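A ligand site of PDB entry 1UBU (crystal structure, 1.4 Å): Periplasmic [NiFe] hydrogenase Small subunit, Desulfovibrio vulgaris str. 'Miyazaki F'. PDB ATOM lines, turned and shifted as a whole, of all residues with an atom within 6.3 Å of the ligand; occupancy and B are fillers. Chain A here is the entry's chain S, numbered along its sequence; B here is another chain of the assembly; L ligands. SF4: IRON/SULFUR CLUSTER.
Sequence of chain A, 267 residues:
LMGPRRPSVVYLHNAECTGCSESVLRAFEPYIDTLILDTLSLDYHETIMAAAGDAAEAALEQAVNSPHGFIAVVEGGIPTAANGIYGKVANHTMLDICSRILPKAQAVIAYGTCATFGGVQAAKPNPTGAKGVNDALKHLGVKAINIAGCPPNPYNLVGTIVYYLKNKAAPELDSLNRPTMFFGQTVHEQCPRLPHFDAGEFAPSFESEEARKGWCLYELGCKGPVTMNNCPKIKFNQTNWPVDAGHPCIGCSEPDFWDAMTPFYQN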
ATOM      1  N   ALA A  15      -8.955 -30.803   8.353  1.00  0.00           N
ATOM      2  CA  ALA A  15     -10.208 -30.049   8.182  1.00  0.00           C
ATOM      3  C   ALA A  15     -10.269 -29.102   9.369  1.00  0.00           C
ATOM      4  O   ALA A  15     -10.601 -29.494  10.467  1.00  0.00           O
ATOM      5  CB  ALA A  15     -11.413 -30.979   8.088  1.00  0.00           C
ATOM      6  N   GLU A  16      -9.949 -27.844   9.102  1.00  0.00           N
ATOM      7  CA  GLU A  16      -9.703 -26.859  10.138  1.00  0.00           C
ATOM      8  C   GLU A  16     -10.042 -25.456   9.631  1.00  0.00           C
ATOM      9  O   GLU A  16     -10.212 -25.252   8.435  1.00  0.00           O
ATOM     10  CB  GLU A  16      -8.242 -26.964  10.611  1.00  0.00           C
ATOM     11  CG  GLU A  16      -7.210 -27.040   9.482  1.00  0.00           C
ATOM     12  CD  GLU A  16      -6.781 -25.722   8.870  1.00  0.00           C
ATOM     13  OE1 GLU A  16      -6.664 -24.686   9.578  1.00  0.00           O
ATOM     14  OE2 GLU A  16      -6.540 -25.723   7.618  1.00  0.00           O
ATOM     15  N   CYS A  17     -10.228 -24.496  10.552  1.00  0.00           N
ATOM     16  CA  CYS A  17     -10.524 -23.134  10.238  1.00  0.00           C
ATOM     17  C   CYS A  17      -9.301 -22.236  10.437  1.00  0.00           C
ATOM     18  O   CYS A  17      -9.395 -21.044  10.146  1.00  0.00           O
ATOM     19  CB  CYS A  17     -11.651 -22.621  11.114  1.00  0.00           C
ATOM     20  SG  CYS A  17     -11.162 -22.166  12.813  1.00  0.00           S
ATOM     21  N   THR A  18      -8.190 -22.792  10.918  1.00  0.00           N
ATOM     22  CA  THR A  18      -6.899 -22.092  11.102  1.00  0.00           C
ATOM     23  C   THR A  18      -6.964 -21.243  12.368  1.00  0.00           C
ATOM     24  O   THR A  18      -5.986 -20.582  12.734  1.00  0.00           O
ATOM     25  CB  THR A  18      -6.469 -21.333   9.841  1.00  0.00           C
ATOM     26  OG1 THR A  18      -6.584 -22.265   8.725  1.00  0.00           O
ATOM     27  CG2 THR A  18      -5.010 -20.887   9.916  1.00  0.00           C
ATOM     28  N   GLY A  19      -8.038 -21.299  13.147  1.00  0.00           N
ATOM     29  CA  GLY A  19      -8.134 -20.621  14.464  1.00  0.00           C
ATOM     30  C   GLY A  19      -7.129 -21.272  15.396  1.00  0.00           C
ATOM     31  O   GLY A  19      -6.603 -20.530  16.265  1.00  0.00           O
ATOM     32  N   CYS A  20      -6.873 -22.569  15.274  1.00  0.00           N
ATOM     33  CA  CYS A  20      -5.886 -23.146  16.195  1.00  0.00           C
ATOM     34  C   CYS A  20      -4.510 -22.637  15.858  1.00  0.00           C
ATOM     35  O   CYS A  20      -3.720 -22.271  16.734  1.00  0.00           O
ATOM     36  CB  CYS A  20      -6.015 -24.687  16.116  1.00  0.00           C
ATOM     37  SG  CYS A  20      -7.430 -25.279  17.056  1.00  0.00           S
ATOM     38  N   SER A  21      -4.124 -22.579  14.568  1.00  0.00           N
ATOM     39  CA  SER A  21      -2.857 -21.978  14.243  1.00  0.00           C
ATOM     40  C   SER A  21      -2.775 -20.536  14.725  1.00  0.00           C
ATOM     41  O   SER A  21      -1.714 -20.152  15.241  1.00  0.00           O
ATOM     42  CB  SER A  21      -2.620 -21.923  12.726  1.00  0.00           C
ATOM     43  OG  SER A  21      -2.367 -23.218  12.181  1.00  0.00           O
ATOM     44  N   GLU A  75      -3.718 -29.991  13.506  1.00  0.00           N
ATOM     45  CA  GLU A  75      -4.906 -29.145  13.632  1.00  0.00           C
ATOM     46  C   GLU A  75      -5.989 -29.661  12.702  1.00  0.00           C
ATOM     47  O   GLU A  75      -5.636 -29.969  11.539  1.00  0.00           O
ATOM     48  CB  GLU A  75      -4.450 -27.706  13.287  1.00  0.00           C
ATOM     49  CG  GLU A  75      -5.621 -26.676  13.168  1.00  0.00           C
ATOM     50  CD  GLU A  75      -5.069 -25.259  12.985  1.00  0.00           C
ATOM     51  OE1 GLU A  75      -5.928 -24.342  12.967  1.00  0.00           O
ATOM     52  OE2 GLU A  75      -3.826 -25.148  12.837  1.00  0.00           O
ATOM     53  N   GLY A  76      -7.243 -29.786  13.136  1.00  0.00           N
ATOM     54  CA  GLY A  76      -8.324 -30.154  12.242  1.00  0.00           C
ATOM     55  C   GLY A  76      -8.634 -31.651  12.344  1.00  0.00           C
ATOM     56  O   GLY A  76      -7.828 -32.536  12.613  1.00  0.00           O
ATOM     57  N   GLY A  77      -9.903 -31.935  12.057  1.00  0.00           N
ATOM     58  CA  GLY A  77     -10.418 -33.292  11.994  1.00  0.00           C
ATOM     59  C   GLY A  77     -10.047 -33.936  10.651  1.00  0.00           C
ATOM     60  O   GLY A  77      -9.711 -33.239   9.703  1.00  0.00           O
ATOM     61  N   TYR A 111      -4.226 -30.753  18.406  1.00  0.00           N
ATOM     62  CA  TYR A 111      -4.422 -29.424  18.955  1.00  0.00           C
ATOM     63  C   TYR A 111      -5.725 -28.855  18.431  1.00  0.00           C
ATOM     64  O   TYR A 111      -5.851 -28.685  17.201  1.00  0.00           O
ATOM     65  CB  TYR A 111      -3.208 -28.540  18.592  1.00  0.00           C
ATOM     66  CG  TYR A 111      -3.281 -27.165  19.246  1.00  0.00           C
ATOM     67  CD1 TYR A 111      -3.279 -27.011  20.641  1.00  0.00           C
ATOM     68  CD2 TYR A 111      -3.391 -26.019  18.448  1.00  0.00           C
ATOM     69  CE1 TYR A 111      -3.371 -25.748  21.247  1.00  0.00           C
ATOM     70  CE2 TYR A 111      -3.477 -24.780  19.038  1.00  0.00           C
ATOM     71  CZ  TYR A 111      -3.465 -24.640  20.408  1.00  0.00           C
ATOM     72  OH  TYR A 111      -3.548 -23.409  21.027  1.00  0.00           O
ATOM     73  N   GLY A 112      -6.659 -28.632  19.351  1.00  0.00           N
ATOM     74  CA  GLY A 112      -7.979 -28.120  19.104  1.00  0.00           C
ATOM     75  C   GLY A 112      -8.998 -29.250  19.047  1.00  0.00           C
ATOM     76  O   GLY A 112      -8.682 -30.394  18.690  1.00  0.00           O
ATOM     77  N   THR A 113     -10.232 -28.918  19.420  1.00  0.00           N
ATOM     78  CA  THR A 113     -11.309 -29.888  19.470  1.00  0.00           C
ATOM     79  C   THR A 113     -11.521 -30.584  18.152  1.00  0.00           C
ATOM     80  O   THR A 113     -11.973 -31.739  18.146  1.00  0.00           O
ATOM     81  CB  THR A 113     -12.589 -29.137  19.952  1.00  0.00           C
ATOM     82  OG1 THR A 113     -12.266 -28.748  21.308  1.00  0.00           O
ATOM     83  CG2 THR A 113     -13.864 -29.981  19.948  1.00  0.00           C
ATOM     84  N   CYS A 114     -11.281 -29.959  17.028  1.00  0.00           N
ATOM     85  CA  CYS A 114     -11.429 -30.708  15.764  1.00  0.00           C
ATOM     86  C   CYS A 114     -10.430 -31.854  15.691  1.00  0.00           C
ATOM     87  O   CYS A 114     -10.803 -33.002  15.400  1.00  0.00           O
ATOM     88  CB  CYS A 114     -11.157 -29.797  14.554  1.00  0.00           C
ATOM     89  SG  CYS A 114     -12.411 -28.464  14.323  1.00  0.00           S
ATOM     90  N   ALA A 115      -9.139 -31.546  15.911  1.00  0.00           N
ATOM     91  CA  ALA A 115      -8.192 -32.655  15.883  1.00  0.00           C
ATOM     92  C   ALA A 115      -8.416 -33.586  17.042  1.00  0.00           C
ATOM     93  O   ALA A 115      -8.155 -34.781  16.935  1.00  0.00           O
ATOM     94  CB  ALA A 115      -6.750 -32.105  15.975  1.00  0.00           C
ATOM     95  N   GLY A 119     -14.760 -32.166  16.095  1.00  0.00           N
ATOM     96  CA  GLY A 119     -15.032 -30.736  15.962  1.00  0.00           C
ATOM     97  C   GLY A 119     -16.178 -30.374  15.062  1.00  0.00           C
ATOM     98  O   GLY A 119     -17.139 -31.122  14.839  1.00  0.00           O
ATOM     99  N   VAL A 120     -16.104 -29.151  14.497  1.00  0.00           N
ATOM    100  CA  VAL A 120     -17.307 -28.520  13.938  1.00  0.00           C
ATOM    101  C   VAL A 120     -17.751 -29.332  12.735  1.00  0.00           C
ATOM    102  O   VAL A 120     -18.955 -29.512  12.561  1.00  0.00           O
ATOM    103  CB  VAL A 120     -17.058 -27.030  13.643  1.00  0.00           C
ATOM    104  CG1 VAL A 120     -16.066 -26.787  12.494  1.00  0.00           C
ATOM    105  CG2 VAL A 120     -18.377 -26.287  13.320  1.00  0.00           C
ATOM    106  N   GLN A 121     -16.861 -29.820  11.896  1.00  0.00           N
ATOM    107  CA  GLN A 121     -17.351 -30.532  10.701  1.00  0.00           C
ATOM    108  C   GLN A 121     -17.849 -31.914  11.075  1.00  0.00           C
ATOM    109  O   GLN A 121     -18.533 -32.539  10.249  1.00  0.00           O
ATOM    110  CB  GLN A 121     -16.272 -30.645   9.610  1.00  0.00           C
ATOM    111  CG  GLN A 121     -14.924 -31.221  10.087  1.00  0.00           C
ATOM    112  CD  GLN A 121     -14.043 -30.190  10.720  1.00  0.00           C
ATOM    113  OE1 GLN A 121     -13.903 -29.053  10.251  1.00  0.00           O
ATOM    114  NE2 GLN A 121     -13.445 -30.488  11.858  1.00  0.00           N
ATOM    115  N   GLY A 149     -10.294 -27.474  22.946  1.00  0.00           N
ATOM    116  CA  GLY A 149     -10.773 -26.107  22.949  1.00  0.00           C
ATOM    117  C   GLY A 149     -10.920 -25.656  21.472  1.00  0.00           C
ATOM    118  O   GLY A 149     -10.306 -26.217  20.554  1.00  0.00           O
ATOM    119  N   CYS A 150     -11.688 -24.592  21.267  1.00  0.00           N
ATOM    120  CA  CYS A 150     -12.031 -24.163  19.924  1.00  0.00           C
ATOM    121  C   CYS A 150     -11.848 -22.663  19.730  1.00  0.00           C
ATOM    122  O   CYS A 150     -12.833 -21.902  19.569  1.00  0.00           O
ATOM    123  CB  CYS A 150     -13.473 -24.578  19.638  1.00  0.00           C
ATOM    124  SG  CYS A 150     -13.959 -24.565  17.881  1.00  0.00           S
ATOM    125  N   PRO A 151     -10.598 -22.204  19.690  1.00  0.00           N
ATOM    126  CA  PRO A 151      -9.367 -22.992  19.855  1.00  0.00           C
ATOM    127  C   PRO A 151      -8.920 -23.085  21.295  1.00  0.00           C
ATOM    128  O   PRO A 151      -9.486 -22.429  22.180  1.00  0.00           O
ATOM    129  CB  PRO A 151      -8.328 -22.145  19.093  1.00  0.00           C
ATOM    130  CG  PRO A 151      -8.826 -20.735  19.367  1.00  0.00           C
ATOM    131  CD  PRO A 151     -10.324 -20.764  19.380  1.00  0.00           C
ATOM    132  N   PRO A 152      -7.976 -23.966  21.583  1.00  0.00           N
ATOM    133  CA  PRO A 152      -7.475 -24.141  22.957  1.00  0.00           C
ATOM    134  C   PRO A 152      -6.745 -22.890  23.399  1.00  0.00           C
ATOM    135  O   PRO A 152      -6.393 -22.035  22.572  1.00  0.00           O
ATOM    136  CB  PRO A 152      -6.425 -25.261  22.835  1.00  0.00           C
ATOM    137  CG  PRO A 152      -6.775 -25.958  21.538  1.00  0.00           C
ATOM    138  CD  PRO A 152      -7.242 -24.849  20.626  1.00  0.00           C
ATOM    139  N   TRP A 258     -20.668 -29.515  19.822  1.00  0.00           N
ATOM    140  CA  TRP A 258     -21.632 -28.880  18.904  1.00  0.00           C
ATOM    141  C   TRP A 258     -23.017 -29.528  18.999  1.00  0.00           C
ATOM    142  O   TRP A 258     -24.023 -28.840  18.729  1.00  0.00           O
ATOM    143  CB  TRP A 258     -21.131 -29.012  17.473  1.00  0.00           C
ATOM    144  CG  TRP A 258     -19.810 -28.314  17.334  1.00  0.00           C
ATOM    145  CD1 TRP A 258     -18.559 -28.870  17.296  1.00  0.00           C
ATOM    146  CD2 TRP A 258     -19.616 -26.913  17.237  1.00  0.00           C
ATOM    147  NE1 TRP A 258     -17.611 -27.886  17.167  1.00  0.00           N
ATOM    148  CE2 TRP A 258     -18.236 -26.670  17.133  1.00  0.00           C
ATOM    149  CE3 TRP A 258     -20.513 -25.832  17.244  1.00  0.00           C
ATOM    150  CZ2 TRP A 258     -17.651 -25.383  17.017  1.00  0.00           C
ATOM    151  CZ3 TRP A 258     -19.964 -24.547  17.131  1.00  0.00           C
ATOM    152  CH2 TRP A 258     -18.580 -24.354  17.024  1.00  0.00           C
ATOM    153  N   ARG B  41     -16.143 -28.826   4.254  1.00  0.00           N
ATOM    154  CA  ARG B  41     -16.600 -29.159   5.584  1.00  0.00           C
ATOM    155  C   ARG B  41     -18.125 -29.258   5.613  1.00  0.00           C
ATOM    156  O   ARG B  41     -18.638 -30.153   6.308  1.00  0.00           O
ATOM    157  CB  ARG B  41     -16.112 -28.151   6.627  1.00  0.00           C
ATOM    158  CG  ARG B  41     -14.632 -28.326   6.905  1.00  0.00           C
ATOM    159  CD  ARG B  41     -14.001 -27.260   7.805  1.00  0.00           C
ATOM    160  NE  ARG B  41     -14.178 -25.967   7.154  1.00  0.00           N
ATOM    161  CZ  ARG B  41     -14.247 -24.796   7.787  1.00  0.00           C
ATOM    162  NH1 ARG B  41     -14.106 -24.715   9.100  1.00  0.00           N
ATOM    163  NH2 ARG B  41     -14.453 -23.693   7.090  1.00  0.00           N
ATOM    164  N   ARG B  61     -16.730 -20.587  13.157  1.00  0.00           N
ATOM    165  CA  ARG B  61     -15.695 -21.596  12.888  1.00  0.00           C
ATOM    166  C   ARG B  61     -15.529 -21.886  11.393  1.00  0.00           C
ATOM    167  O   ARG B  61     -14.795 -22.777  10.962  1.00  0.00           O
ATOM    168  CB  ARG B  61     -15.982 -22.912  13.644  1.00  0.00           C
ATOM    169  CG  ARG B  61     -15.502 -22.870  15.085  1.00  0.00           C
ATOM    170  CD  ARG B  61     -16.273 -21.815  15.902  1.00  0.00           C
ATOM    171  NE  ARG B  61     -15.758 -21.866  17.275  1.00  0.00           N
ATOM    172  CZ  ARG B  61     -16.206 -21.114  18.268  1.00  0.00           C
ATOM    173  NH1 ARG B  61     -17.245 -20.278  18.090  1.00  0.00           N
ATOM    174  NH2 ARG B  61     -15.621 -21.198  19.461  1.00  0.00           N
ATOM    175  N   GLY B  64     -10.790 -18.978  11.406  1.00  0.00           N
ATOM    176  CA  GLY B  64     -10.132 -18.369  12.572  1.00  0.00           C
ATOM    177  C   GLY B  64      -9.107 -17.303  12.208  1.00  0.00           C
ATOM    178  O   GLY B  64      -8.528 -16.716  13.137  1.00  0.00           O
ATOM    179  N   PRO B 216      -8.322 -16.160  19.159  1.00  0.00           N
ATOM    180  CA  PRO B 216      -9.418 -16.255  18.212  1.00  0.00           C
ATOM    181  C   PRO B 216     -10.747 -16.692  18.822  1.00  0.00           C
ATOM    182  O   PRO B 216     -10.810 -17.302  19.904  1.00  0.00           O
ATOM    183  CB  PRO B 216      -8.968 -17.355  17.203  1.00  0.00           C
ATOM    184  CG  PRO B 216      -7.485 -17.456  17.406  1.00  0.00           C
ATOM    185  CD  PRO B 216      -7.294 -17.201  18.893  1.00  0.00           C
ATOM    186  N   HIS B 217     -11.795 -16.396  18.052  1.00  0.00           N
ATOM    187  CA  HIS B 217     -13.193 -16.774  18.165  1.00  0.00           C
ATOM    188  C   HIS B 217     -13.795 -16.059  19.359  1.00  0.00           C
ATOM    189  O   HIS B 217     -13.855 -16.524  20.488  1.00  0.00           O
ATOM    190  CB  HIS B 217     -13.356 -18.310  18.235  1.00  0.00           C
ATOM    191  CG  HIS B 217     -13.105 -18.910  16.872  1.00  0.00           C
ATOM    192  ND1 HIS B 217     -12.834 -20.196  16.586  1.00  0.00           N
ATOM    193  CD2 HIS B 217     -13.082 -18.205  15.683  1.00  0.00           C
ATOM    194  CE1 HIS B 217     -12.658 -20.330  15.244  1.00  0.00           C
ATOM    195  NE2 HIS B 217     -12.806 -19.116  14.715  1.00  0.00           N
HETATM  196 FE1  SF4 L   1     -11.068 -24.016  14.169  1.00  0.00          FE
HETATM  197 FE2  SF4 L   1     -11.339 -26.573  14.806  1.00  0.00          FE
HETATM  198 FE3  SF4 L   1     -12.105 -24.724  16.518  1.00  0.00          FE
HETATM  199 FE4  SF4 L   1      -9.448 -25.055  16.028  1.00  0.00          FE
HETATM  200  S1  SF4 L   1     -10.824 -26.570  17.052  1.00  0.00           S
HETATM  201  S2  SF4 L   1     -10.620 -23.139  16.237  1.00  0.00           S
HETATM  202  S3  SF4 L   1      -9.510 -25.678  13.795  1.00  0.00           S
HETATM  203  S4  SF4 L   1     -13.044 -25.100  14.420  1.00  0.00           S
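The backbone NH of Cys 114 sits close to a sulfur (S1) of the ligand, 3.4 Å away.
The side-chain sulfur (SG) of Cys 114 binds an iron atom (FE2) of the ligand (2.2 Å).
An iron atom (FE4) of the ligand is bound by the side-chain sulfur (SG) of Cys 20, 2.3 Å away.
The backbone NH of Cys 17 lies close to a sulfur (S3) of the ligand, at 3.5 Å.
An iron atom (FE1) of the ligand is bound by the side-chain sulfur (SG) of Cys 17 (2.3 Å).
SG of Cys 150 binds FE3 of the ligand, 2.3 Å away.
N of Thr 113 lies close to S1 of the ligand (3.4 Å).
A sulfur (S2) of the ligand sits close to a ring nitrogen (ND1) of His 217 of chain B (3.7 Å).
The side-chain sulfur of Cys 114 sits close to the backbone NH of Val 120 (3.8 Å).
The side-chain sulfur of Cys 114 lies close to the side-chain amide nitrogen of Gln 121, at 3.4 Å.
N of Cys 20 is in hydrogen-bond range of OE1 of Glu 75 (3.1 Å).
SG of Cys 20 lies close to O of Tyr 111, 3.8 Å away.
N of Gly 19 lies close to SG of Cys 17, 3.3 Å away.
The backbone carbonyl oxygen (O) of Cys 150 lies within hydrogen-bond range of the guanidinium group (NH2) of Arg 61 of chain B (2.9 Å).
NE of Arg 61 of chain B lies within hydrogen-bond range of ND1 of His 217 of chain B (3.4 Å).
N of Thr 18 sits close to OE1 of Glu 75 (3.4 Å).
A sulfur (S1) of the ligand lies close to the backbone carbonyl oxygen of Gly 149 (3.6 Å).
The backbone nitrogen (N) of Pro 151 lies close to a sulfur (S2) of the ligand, 3.6 Å away.
Merely in contact with the ligand: Arg 61 of chain B (3.4 Å), Glu 16 (3.7 Å), Gly 112 (3.8 Å), Glu 75 (3.9 Å), Gly 19 (3.96 Å) and Val 120 (3.96 Å).
Hydrophobic or aromatic side chains within 4 Å of the ligand: Val 120, Pro 151 and His 217 of chain B.
Within 4 Å of the ligand: Glu 16, Cys 17, Gly 19, Cys 20, Glu 75, Gly 112, Thr 113, Cys 114, Val 120, Gly 149, Cys 150, Pro 151, Arg 61 of chain B and His 217 of chain B.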
